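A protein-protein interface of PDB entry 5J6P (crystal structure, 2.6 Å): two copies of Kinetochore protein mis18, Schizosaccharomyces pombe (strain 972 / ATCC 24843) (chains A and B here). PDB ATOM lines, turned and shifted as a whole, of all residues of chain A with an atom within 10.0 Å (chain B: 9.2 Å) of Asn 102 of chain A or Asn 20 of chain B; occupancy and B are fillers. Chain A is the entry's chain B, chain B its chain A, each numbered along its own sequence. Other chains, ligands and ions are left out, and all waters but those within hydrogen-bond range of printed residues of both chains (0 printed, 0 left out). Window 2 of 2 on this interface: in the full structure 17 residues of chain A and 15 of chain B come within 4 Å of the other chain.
The side-chain carboxylate (OD2) of Asp 18 of chain B sits at hydrogen-bond distance from the side-chain hydroxyl (OH) of Tyr 98 of chain A, 2.4 Å away.
The backbone NH (N) of Gly 101 of chain A sits at hydrogen-bond distance from the side-chain carboxylate (OD2) of Asp 18 of chain B (3.3 Å).
ND2 of Asn 20 of chain B lies within hydrogen-bond range of OE1 of Gln 3 of chain A.
The side-chain amide nitrogen (ND2) of Asn 20 of chain B lies within hydrogen-bond range of the backbone carbonyl oxygen (O) of Gly 101 of chain A (2.6 Å).
The backbone carbonyl oxygen (O) of Gln 3 of chain A lies within hydrogen-bond range of the side-chain amide nitrogen (NE2) of Gln 99 of chain A (2.9 Å).
The backbone carbonyl oxygen of Gly 17 of chain B is in hydrogen-bond range of the backbone NH of Phe 7 of chain B (2.8 Å).
O of Pro 4 of chain B sits at hydrogen-bond distance from N of Leu 100 of chain B (3.1 Å).
The backbone NH of Asn 20 of chain B sits at hydrogen-bond distance from the side-chain carboxylate of Asp 18 of chain B (3.0 Å).
The backbone carbonyl oxygen (O) of Pro 4 of chain A sits at hydrogen-bond distance from the backbone NH (N) of Leu 100 of chain A (3.1 Å).
CB of Pro 4 of chain A touches CD2 of Leu 100 of chain B (3.4 Å).
Tyr 98 of chain A touches Val 6 of chain B.
CA of Gly 17 of chain B touches OH of Tyr 98 of chain A, at 3.7 Å.
Pro 4 of chain B touches Leu 100 of chain A.
Leu 100 of chain A touches Val 6 of chain B.
OD2 of Asp 18 of chain B touches CA of Leu 100 of chain A (3.3 Å).
C of Asn 102 of chain A touches CB of Asn 20 of chain B, at 3.8 Å.
Of the printed residues of chain B, Pro 4 of chain A touches Leu 100 (3.4 Å).
Gly 101 of chain A touches just these residues of chain B: Asp 18 (3.3 Å) and Asn 20 (2.6 Å).
Of the printed residues of chain A, Gly 17 of chain B touches Tyr 98 (3.7 Å).
Of chain A, only Tyr 98 (2.4 Å), Leu 100 (3.3 Å) and Gly 101 (3.3 Å) come within 4 Å of Asp 18 of chain B.
Printed residues of chain A within 4 Å of Asn 20 of chain B: Gln 3, Gly 101 and Asn 102.
No residue of chain A comes within 4 Å of Ala 21 of chain B.
Printed residues of chain A within 4 Å of Leu 100 of chain B: Pro 4.
The nearest residue of chain B that does not touch Asn 102 of chain A is Asp 18 of chain B (5.5 Å).
The nearest residue of chain A that does not touch Asn 20 of chain B is Leu 100 of chain A (4.04 Å).
The nearest printed residue of chain B that does not touch Gln 3 of chain A is Pro 4 of chain B (5.5 Å).
Of the 19 printed residues of chain B, 6 touch a printed residue of chain A.
Hydrophobic or aromatic side chains of chain B that line the printed part of chain A: Pro 4, Val 6 and Leu 100.
Hydrophobic or aromatic side chains of chain A within 4 Å of the printed part of chain B: Pro 4, Tyr 98 and Leu 100.
Among the printed residues, no Asp or Glu carboxylate lies within 4 Å of a Lys or Arg side-chain nitrogen of the other chain.
Pro 4 of chain A touches Leu 100 of chain B, and with the chains exchanged Leu 100 of chain A touches Pro 4 of chain B.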
ATOM      1  N   GLU A   1       9.687 -23.681  15.706  1.00  0.00           N
ATOM      2  CA  GLU A   1       9.662 -22.256  15.211  1.00  0.00           C
ATOM      3  C   GLU A   1      11.054 -21.811  14.740  1.00  0.00           C
ATOM      4  O   GLU A   1      11.648 -20.881  15.296  1.00  0.00           O
ATOM      5  CB  GLU A   1       9.027 -21.248  16.222  1.00  0.00           C
ATOM      6  CG  GLU A   1       9.181 -21.543  17.720  1.00  0.00           C
ATOM      7  CD  GLU A   1       8.129 -22.525  18.295  1.00  0.00           C
ATOM      8  OE1 GLU A   1       8.177 -22.818  19.517  1.00  0.00           O
ATOM      9  OE2 GLU A   1       7.252 -23.023  17.546  1.00  0.00           O
ATOM     10  N   SER A   2      11.569 -22.513  13.722  1.00  0.00           N
ATOM     11  CA  SER A   2      12.837 -22.171  13.026  1.00  0.00           C
ATOM     12  C   SER A   2      14.118 -22.108  13.909  1.00  0.00           C
ATOM     13  O   SER A   2      15.221 -21.765  13.424  1.00  0.00           O
ATOM     14  CB  SER A   2      12.664 -20.871  12.193  1.00  0.00           C
ATOM     15  OG  SER A   2      12.234 -19.771  12.982  1.00  0.00           O
ATOM     16  N   GLN A   3      13.986 -22.493  15.178  1.00  0.00           N
ATOM     17  CA  GLN A   3      15.062 -22.337  16.150  1.00  0.00           C
ATOM     18  C   GLN A   3      15.655 -23.725  16.438  1.00  0.00           C
ATOM     19  O   GLN A   3      14.888 -24.667  16.668  1.00  0.00           O
ATOM     20  CB  GLN A   3      14.544 -21.662  17.433  1.00  0.00           C
ATOM     21  CG  GLN A   3      15.620 -20.874  18.179  1.00  0.00           C
ATOM     22  CD  GLN A   3      16.211 -19.733  17.357  1.00  0.00           C
ATOM     23  OE1 GLN A   3      17.403 -19.714  17.030  1.00  0.00           O
ATOM     24  NE2 GLN A   3      15.369 -18.782  17.003  1.00  0.00           N
ATOM     25  N   PRO A   4      17.005 -23.852  16.413  1.00  0.00           N
ATOM     26  CA  PRO A   4      17.662 -25.143  16.682  1.00  0.00           C
ATOM     27  C   PRO A   4      17.312 -25.808  18.031  1.00  0.00           C
ATOM     28  O   PRO A   4      16.878 -25.130  18.981  1.00  0.00           O
ATOM     29  CB  PRO A   4      19.175 -24.797  16.657  1.00  0.00           C
ATOM     30  CG  PRO A   4      19.277 -23.515  15.889  1.00  0.00           C
ATOM     31  CD  PRO A   4      18.009 -22.776  16.233  1.00  0.00           C
ATOM     32  N   SER A   5      17.477 -27.130  18.079  1.00  0.00           N
ATOM     33  CA  SER A   5      17.601 -27.856  19.337  1.00  0.00           C
ATOM     34  C   SER A   5      19.014 -28.420  19.593  1.00  0.00           C
ATOM     35  O   SER A   5      19.854 -28.531  18.684  1.00  0.00           O
ATOM     36  CB  SER A   5      16.543 -28.944  19.428  1.00  0.00           C
ATOM     37  OG  SER A   5      15.230 -28.388  19.431  1.00  0.00           O
ATOM     38  N   TYR A  98      16.713 -29.635  23.878  1.00  0.00           N
ATOM     39  CA  TYR A  98      16.571 -28.312  24.373  1.00  0.00           C
ATOM     40  C   TYR A  98      16.530 -27.425  23.145  1.00  0.00           C
ATOM     41  O   TYR A  98      17.561 -27.277  22.424  1.00  0.00           O
ATOM     42  CB  TYR A  98      17.730 -27.938  25.312  1.00  0.00           C
ATOM     43  CG  TYR A  98      17.751 -26.456  25.576  1.00  0.00           C
ATOM     44  CD1 TYR A  98      16.810 -25.868  26.449  1.00  0.00           C
ATOM     45  CD2 TYR A  98      18.659 -25.627  24.915  1.00  0.00           C
ATOM     46  CE1 TYR A  98      16.784 -24.494  26.644  1.00  0.00           C
ATOM     47  CE2 TYR A  98      18.651 -24.262  25.121  1.00  0.00           C
ATOM     48  CZ  TYR A  98      17.712 -23.705  25.966  1.00  0.00           C
ATOM     49  OH  TYR A  98      17.704 -22.357  26.127  1.00  0.00           O
ATOM     50  N   GLN A  99      15.338 -26.858  22.907  1.00  0.00           N
ATOM     51  CA  GLN A  99      15.157 -25.882  21.835  1.00  0.00           C
ATOM     52  C   GLN A  99      15.456 -24.518  22.394  1.00  0.00           C
ATOM     53  O   GLN A  99      14.843 -24.120  23.372  1.00  0.00           O
ATOM     54  CB  GLN A  99      13.745 -25.896  21.239  1.00  0.00           C
ATOM     55  CG  GLN A  99      13.739 -25.239  19.851  1.00  0.00           C
ATOM     56  CD  GLN A  99      12.351 -24.997  19.269  1.00  0.00           C
ATOM     57  OE1 GLN A  99      11.330 -25.318  19.889  1.00  0.00           O
ATOM     58  NE2 GLN A  99      12.315 -24.409  18.066  1.00  0.00           N
ATOM     59  N   LEU A 100      16.360 -23.798  21.749  1.00  0.00           N
ATOM     60  CA  LEU A 100      16.738 -22.455  22.187  1.00  0.00           C
ATOM     61  C   LEU A 100      15.544 -21.481  22.093  1.00  0.00           C
ATOM     62  O   LEU A 100      14.569 -21.774  21.408  1.00  0.00           O
ATOM     63  CB  LEU A 100      17.880 -21.897  21.334  1.00  0.00           C
ATOM     64  CG  LEU A 100      19.278 -22.487  21.487  1.00  0.00           C
ATOM     65  CD1 LEU A 100      19.322 -23.986  21.275  1.00  0.00           C
ATOM     66  CD2 LEU A 100      20.237 -21.802  20.522  1.00  0.00           C
ATOM     67  N   GLY A 101      15.623 -20.355  22.813  1.00  0.00           N
ATOM     68  CA  GLY A 101      14.650 -19.252  22.713  1.00  0.00           C
ATOM     69  C   GLY A 101      15.102 -18.275  21.626  1.00  0.00           C
ATOM     70  O   GLY A 101      16.105 -18.538  20.897  1.00  0.00           O
ATOM     71  N   ASN A 102      14.422 -17.118  21.568  1.00  0.00           N
ATOM     72  CA  ASN A 102      14.380 -16.265  20.350  1.00  0.00           C
ATOM     73  C   ASN A 102      15.310 -15.038  20.307  1.00  0.00           C
ATOM     74  O   ASN A 102      15.541 -14.457  19.229  1.00  0.00           O
ATOM     75  CB  ASN A 102      12.928 -15.815  20.088  1.00  0.00           C
ATOM     76  CG  ASN A 102      11.917 -16.961  20.207  1.00  0.00           C
ATOM     77  OD1 ASN A 102      10.917 -16.849  20.907  1.00  0.00           O
ATOM     78  ND2 ASN A 102      12.183 -18.064  19.526  1.00  0.00           N
ATOM     79  N   SER B   2      28.828 -16.114  14.693  1.00  0.00           N
ATOM     80  CA  SER B   2      28.385 -17.017  13.595  1.00  0.00           C
ATOM     81  C   SER B   2      27.120 -17.789  14.022  1.00  0.00           C
ATOM     82  O   SER B   2      26.022 -17.536  13.526  1.00  0.00           O
ATOM     83  CB  SER B   2      29.537 -17.973  13.211  1.00  0.00           C
ATOM     84  OG  SER B   2      29.190 -18.763  12.092  1.00  0.00           O
ATOM     85  N   GLN B   3      27.304 -18.673  14.999  1.00  0.00           N
ATOM     86  CA  GLN B   3      26.353 -19.717  15.357  1.00  0.00           C
ATOM     87  C   GLN B   3      26.213 -19.734  16.887  1.00  0.00           C
ATOM     88  O   GLN B   3      27.229 -19.756  17.597  1.00  0.00           O
ATOM     89  CB  GLN B   3      26.906 -21.063  14.847  1.00  0.00           C
ATOM     90  CG  GLN B   3      25.911 -22.221  14.819  1.00  0.00           C
ATOM     91  CD  GLN B   3      24.826 -22.086  13.752  1.00  0.00           C
ATOM     92  OE1 GLN B   3      25.134 -22.030  12.572  1.00  0.00           O
ATOM     93  NE2 GLN B   3      23.555 -22.062  14.162  1.00  0.00           N
ATOM     94  N   PRO B   4      24.972 -19.755  17.403  1.00  0.00           N
ATOM     95  CA  PRO B   4      24.805 -19.498  18.801  1.00  0.00           C
ATOM     96  C   PRO B   4      25.292 -20.622  19.704  1.00  0.00           C
ATOM     97  O   PRO B   4      25.653 -21.730  19.238  1.00  0.00           O
ATOM     98  CB  PRO B   4      23.294 -19.387  18.934  1.00  0.00           C
ATOM     99  CG  PRO B   4      22.783 -20.403  17.978  1.00  0.00           C
ATOM    100  CD  PRO B   4      23.739 -20.300  16.815  1.00  0.00           C
ATOM    101  N   SER B   5      25.283 -20.306  20.998  1.00  0.00           N
ATOM    102  CA  SER B   5      25.674 -21.222  22.048  1.00  0.00           C
ATOM    103  C   SER B   5      24.593 -21.469  23.062  1.00  0.00           C
ATOM    104  O   SER B   5      23.671 -20.668  23.251  1.00  0.00           O
ATOM    105  CB  SER B   5      26.892 -20.702  22.772  1.00  0.00           C
ATOM    106  OG  SER B   5      27.908 -20.502  21.825  1.00  0.00           O
ATOM    107  N   VAL B   6      24.762 -22.611  23.716  1.00  0.00           N
ATOM    108  CA  VAL B   6      23.987 -23.041  24.859  1.00  0.00           C
ATOM    109  C   VAL B   6      24.989 -23.042  26.040  1.00  0.00           C
ATOM    110  O   VAL B   6      26.226 -23.120  25.834  1.00  0.00           O
ATOM    111  CB  VAL B   6      23.394 -24.416  24.515  1.00  0.00           C
ATOM    112  CG1 VAL B   6      23.551 -25.441  25.633  1.00  0.00           C
ATOM    113  CG2 VAL B   6      21.948 -24.271  24.077  1.00  0.00           C
ATOM    114  N   PHE B   7      24.472 -22.922  27.258  1.00  0.00           N
ATOM    115  CA  PHE B   7      25.315 -22.820  28.463  1.00  0.00           C
ATOM    116  C   PHE B   7      24.900 -23.846  29.524  1.00  0.00           C
ATOM    117  O   PHE B   7      23.707 -24.001  29.794  1.00  0.00           O
ATOM    118  CB  PHE B   7      25.171 -21.424  29.079  1.00  0.00           C
ATOM    119  CG  PHE B   7      25.528 -20.295  28.148  1.00  0.00           C
ATOM    120  CD1 PHE B   7      26.857 -20.077  27.779  1.00  0.00           C
ATOM    121  CD2 PHE B   7      24.534 -19.439  27.639  1.00  0.00           C
ATOM    122  CE1 PHE B   7      27.207 -19.046  26.925  1.00  0.00           C
ATOM    123  CE2 PHE B   7      24.878 -18.402  26.780  1.00  0.00           C
ATOM    124  CZ  PHE B   7      26.218 -18.204  26.427  1.00  0.00           C
ATOM    125  N   GLY B  17      20.578 -21.845  29.860  1.00  0.00           N
ATOM    126  CA  GLY B  17      19.967 -21.066  28.777  1.00  0.00           C
ATOM    127  C   GLY B  17      20.977 -20.867  27.654  1.00  0.00           C
ATOM    128  O   GLY B  17      21.982 -21.598  27.586  1.00  0.00           O
ATOM    129  N   ASP B  18      20.756 -19.853  26.806  1.00  0.00           N
ATOM    130  CA  ASP B  18      21.556 -19.695  25.569  1.00  0.00           C
ATOM    131  C   ASP B  18      21.867 -18.273  25.154  1.00  0.00           C
ATOM    132  O   ASP B  18      21.313 -17.325  25.680  1.00  0.00           O
ATOM    133  CB  ASP B  18      20.824 -20.387  24.413  1.00  0.00           C
ATOM    134  CG  ASP B  18      19.369 -19.954  24.282  1.00  0.00           C
ATOM    135  OD1 ASP B  18      19.098 -18.754  24.016  1.00  0.00           O
ATOM    136  OD2 ASP B  18      18.493 -20.831  24.429  1.00  0.00           O
ATOM    137  N   SER B  19      22.757 -18.161  24.180  1.00  0.00           N
ATOM    138  CA  SER B  19      23.044 -16.925  23.450  1.00  0.00           C
ATOM    139  C   SER B  19      21.887 -15.985  23.132  1.00  0.00           C
ATOM    140  O   SER B  19      22.034 -14.760  23.178  1.00  0.00           O
ATOM    141  CB  SER B  19      23.620 -17.298  22.096  1.00  0.00           C
ATOM    142  OG  SER B  19      24.972 -17.640  22.255  1.00  0.00           O
ATOM    143  N   ASN B  20      20.748 -16.531  22.750  1.00  0.00           N
ATOM    144  CA  ASN B  20      19.683 -15.662  22.239  1.00  0.00           C
ATOM    145  C   ASN B  20      18.955 -14.813  23.249  1.00  0.00           C
ATOM    146  O   ASN B  20      18.088 -14.030  22.862  1.00  0.00           O
ATOM    147  CB  ASN B  20      18.647 -16.488  21.505  1.00  0.00           C
ATOM    148  CG  ASN B  20      19.248 -17.279  20.378  1.00  0.00           C
ATOM    149  OD1 ASN B  20      20.449 -17.101  20.014  1.00  0.00           O
ATOM    150  ND2 ASN B  20      18.437 -18.187  19.832  1.00  0.00           N
ATOM    151  N   ALA B  21      19.253 -15.010  24.531  1.00  0.00           N
ATOM    152  CA  ALA B  21      18.782 -14.130  25.579  1.00  0.00           C
ATOM    153  C   ALA B  21      19.908 -13.256  26.138  1.00  0.00           C
ATOM    154  O   ALA B  21      19.707 -12.602  27.161  1.00  0.00           O
ATOM    155  CB  ALA B  21      18.127 -14.945  26.685  1.00  0.00           C
ATOM    156  N   TRP B  22      21.057 -13.197  25.453  1.00  0.00           N
ATOM    157  CA  TRP B  22      22.208 -12.395  25.898  1.00  0.00           C
ATOM    158  C   TRP B  22      21.865 -10.927  25.968  1.00  0.00           C
ATOM    159  O   TRP B  22      21.027 -10.442  25.198  1.00  0.00           O
ATOM    160  CB  TRP B  22      23.370 -12.557  24.934  1.00  0.00           C
ATOM    161  CG  TRP B  22      24.645 -11.859  25.219  1.00  0.00           C
ATOM    162  CD1 TRP B  22      24.921 -10.569  24.971  1.00  0.00           C
ATOM    163  CD2 TRP B  22      25.855 -12.452  25.694  1.00  0.00           C
ATOM    164  NE1 TRP B  22      26.220 -10.270  25.330  1.00  0.00           N
ATOM    165  CE2 TRP B  22      26.831 -11.412  25.763  1.00  0.00           C
ATOM    166  CE3 TRP B  22      26.220 -13.755  26.079  1.00  0.00           C
ATOM    167  CZ2 TRP B  22      28.171 -11.630  26.204  1.00  0.00           C
ATOM    168  CZ3 TRP B  22      27.568 -13.988  26.519  1.00  0.00           C
ATOM    169  CH2 TRP B  22      28.524 -12.923  26.573  1.00  0.00           C
ATOM    170  N   VAL B  23      22.498 -10.265  26.942  1.00  0.00           N
ATOM    171  CA  VAL B  23      22.376  -8.840  27.189  1.00  0.00           C
ATOM    172  C   VAL B  23      23.770  -8.208  27.121  1.00  0.00           C
ATOM    173  O   VAL B  23      24.028  -7.329  26.295  1.00  0.00           O
ATOM    174  CB  VAL B  23      21.756  -8.585  28.581  1.00  0.00           C
ATOM    175  CG1 VAL B  23      21.829  -7.102  28.996  1.00  0.00           C
ATOM    176  CG2 VAL B  23      20.333  -9.111  28.608  1.00  0.00           C
ATOM    177  N   THR B  33      25.428 -11.928  31.204  1.00  0.00           N
ATOM    178  CA  THR B  33      24.093 -11.653  31.633  1.00  0.00           C
ATOM    179  C   THR B  33      23.085 -11.938  30.538  1.00  0.00           C
ATOM    180  O   THR B  33      23.194 -11.453  29.421  1.00  0.00           O
ATOM    181  CB  THR B  33      23.972 -10.212  32.254  1.00  0.00           C
ATOM    182  OG1 THR B  33      24.818 -10.125  33.422  1.00  0.00           O
ATOM    183  CG2 THR B  33      22.525  -9.892  32.683  1.00  0.00           C
ATOM    184  N   LEU B  34      22.095 -12.740  30.898  1.00  0.00           N
ATOM    185  CA  LEU B  34      21.016 -13.104  30.020  1.00  0.00           C
ATOM    186  C   LEU B  34      19.735 -12.525  30.579  1.00  0.00           C
ATOM    187  O   LEU B  34      19.644 -12.220  31.751  1.00  0.00           O
ATOM    188  CB  LEU B  34      20.860 -14.627  29.962  1.00  0.00           C
ATOM    189  CG  LEU B  34      21.738 -15.467  29.038  1.00  0.00           C
ATOM    190  CD1 LEU B  34      23.221 -15.265  29.252  1.00  0.00           C
ATOM    191  CD2 LEU B  34      21.370 -16.932  29.246  1.00  0.00           C
ATOM    192  N   SER B  35      18.739 -12.435  29.717  1.00  0.00           N
ATOM    193  CA  SER B  35      17.450 -11.907  30.058  1.00  0.00           C
ATOM    194  C   SER B  35      16.525 -13.005  30.392  1.00  0.00           C
ATOM    195  O   SER B  35      15.413 -12.759  30.843  1.00  0.00           O
ATOM    196  CB  SER B  35      16.868 -11.088  28.888  1.00  0.00           C
ATOM    197  OG  SER B  35      17.166 -11.669  27.621  1.00  0.00           O
ATOM    198  N   ASP B  36      16.943 -14.236  30.147  1.00  0.00           N
ATOM    199  CA  ASP B  36      16.055 -15.367  30.338  1.00  0.00           C
ATOM    200  C   ASP B  36      16.850 -16.637  30.566  1.00  0.00           C
ATOM    201  O   ASP B  36      18.031 -16.751  30.191  1.00  0.00           O
ATOM    202  CB  ASP B  36      15.130 -15.503  29.123  1.00  0.00           C
ATOM    203  CG  ASP B  36      13.890 -16.303  29.422  1.00  0.00           C
ATOM    204  OD1 ASP B  36      13.520 -16.396  30.614  1.00  0.00           O
ATOM    205  OD2 ASP B  36      13.293 -16.857  28.464  1.00  0.00           O
ATOM    206  N   ALA B  37      16.195 -17.590  31.199  1.00  0.00           N
ATOM    207  CA  ALA B  37      16.853 -18.801  31.616  1.00  0.00           C
ATOM    208  C   ALA B  37      15.812 -19.828  31.943  1.00  0.00           C
ATOM    209  O   ALA B  37      14.691 -19.480  32.299  1.00  0.00           O
ATOM    210  CB  ALA B  37      17.696 -18.527  32.859  1.00  0.00           C
ATOM    211  N   LEU B 100      26.960 -24.500  18.527  1.00  0.00           N
ATOM    212  CA  LEU B 100      26.316 -25.442  17.589  1.00  0.00           C
ATOM    213  C   LEU B 100      27.026 -25.839  16.268  1.00  0.00           C
ATOM    214  O   LEU B 100      26.681 -26.875  15.673  1.00  0.00           O
ATOM    215  CB  LEU B 100      24.896 -24.976  17.245  1.00  0.00           C
ATOM    216  CG  LEU B 100      23.793 -25.336  18.226  1.00  0.00           C
ATOM    217  CD1 LEU B 100      23.989 -24.663  19.568  1.00  0.00           C
ATOM    218  CD2 LEU B 100      22.431 -24.954  17.702  1.00  0.00           C
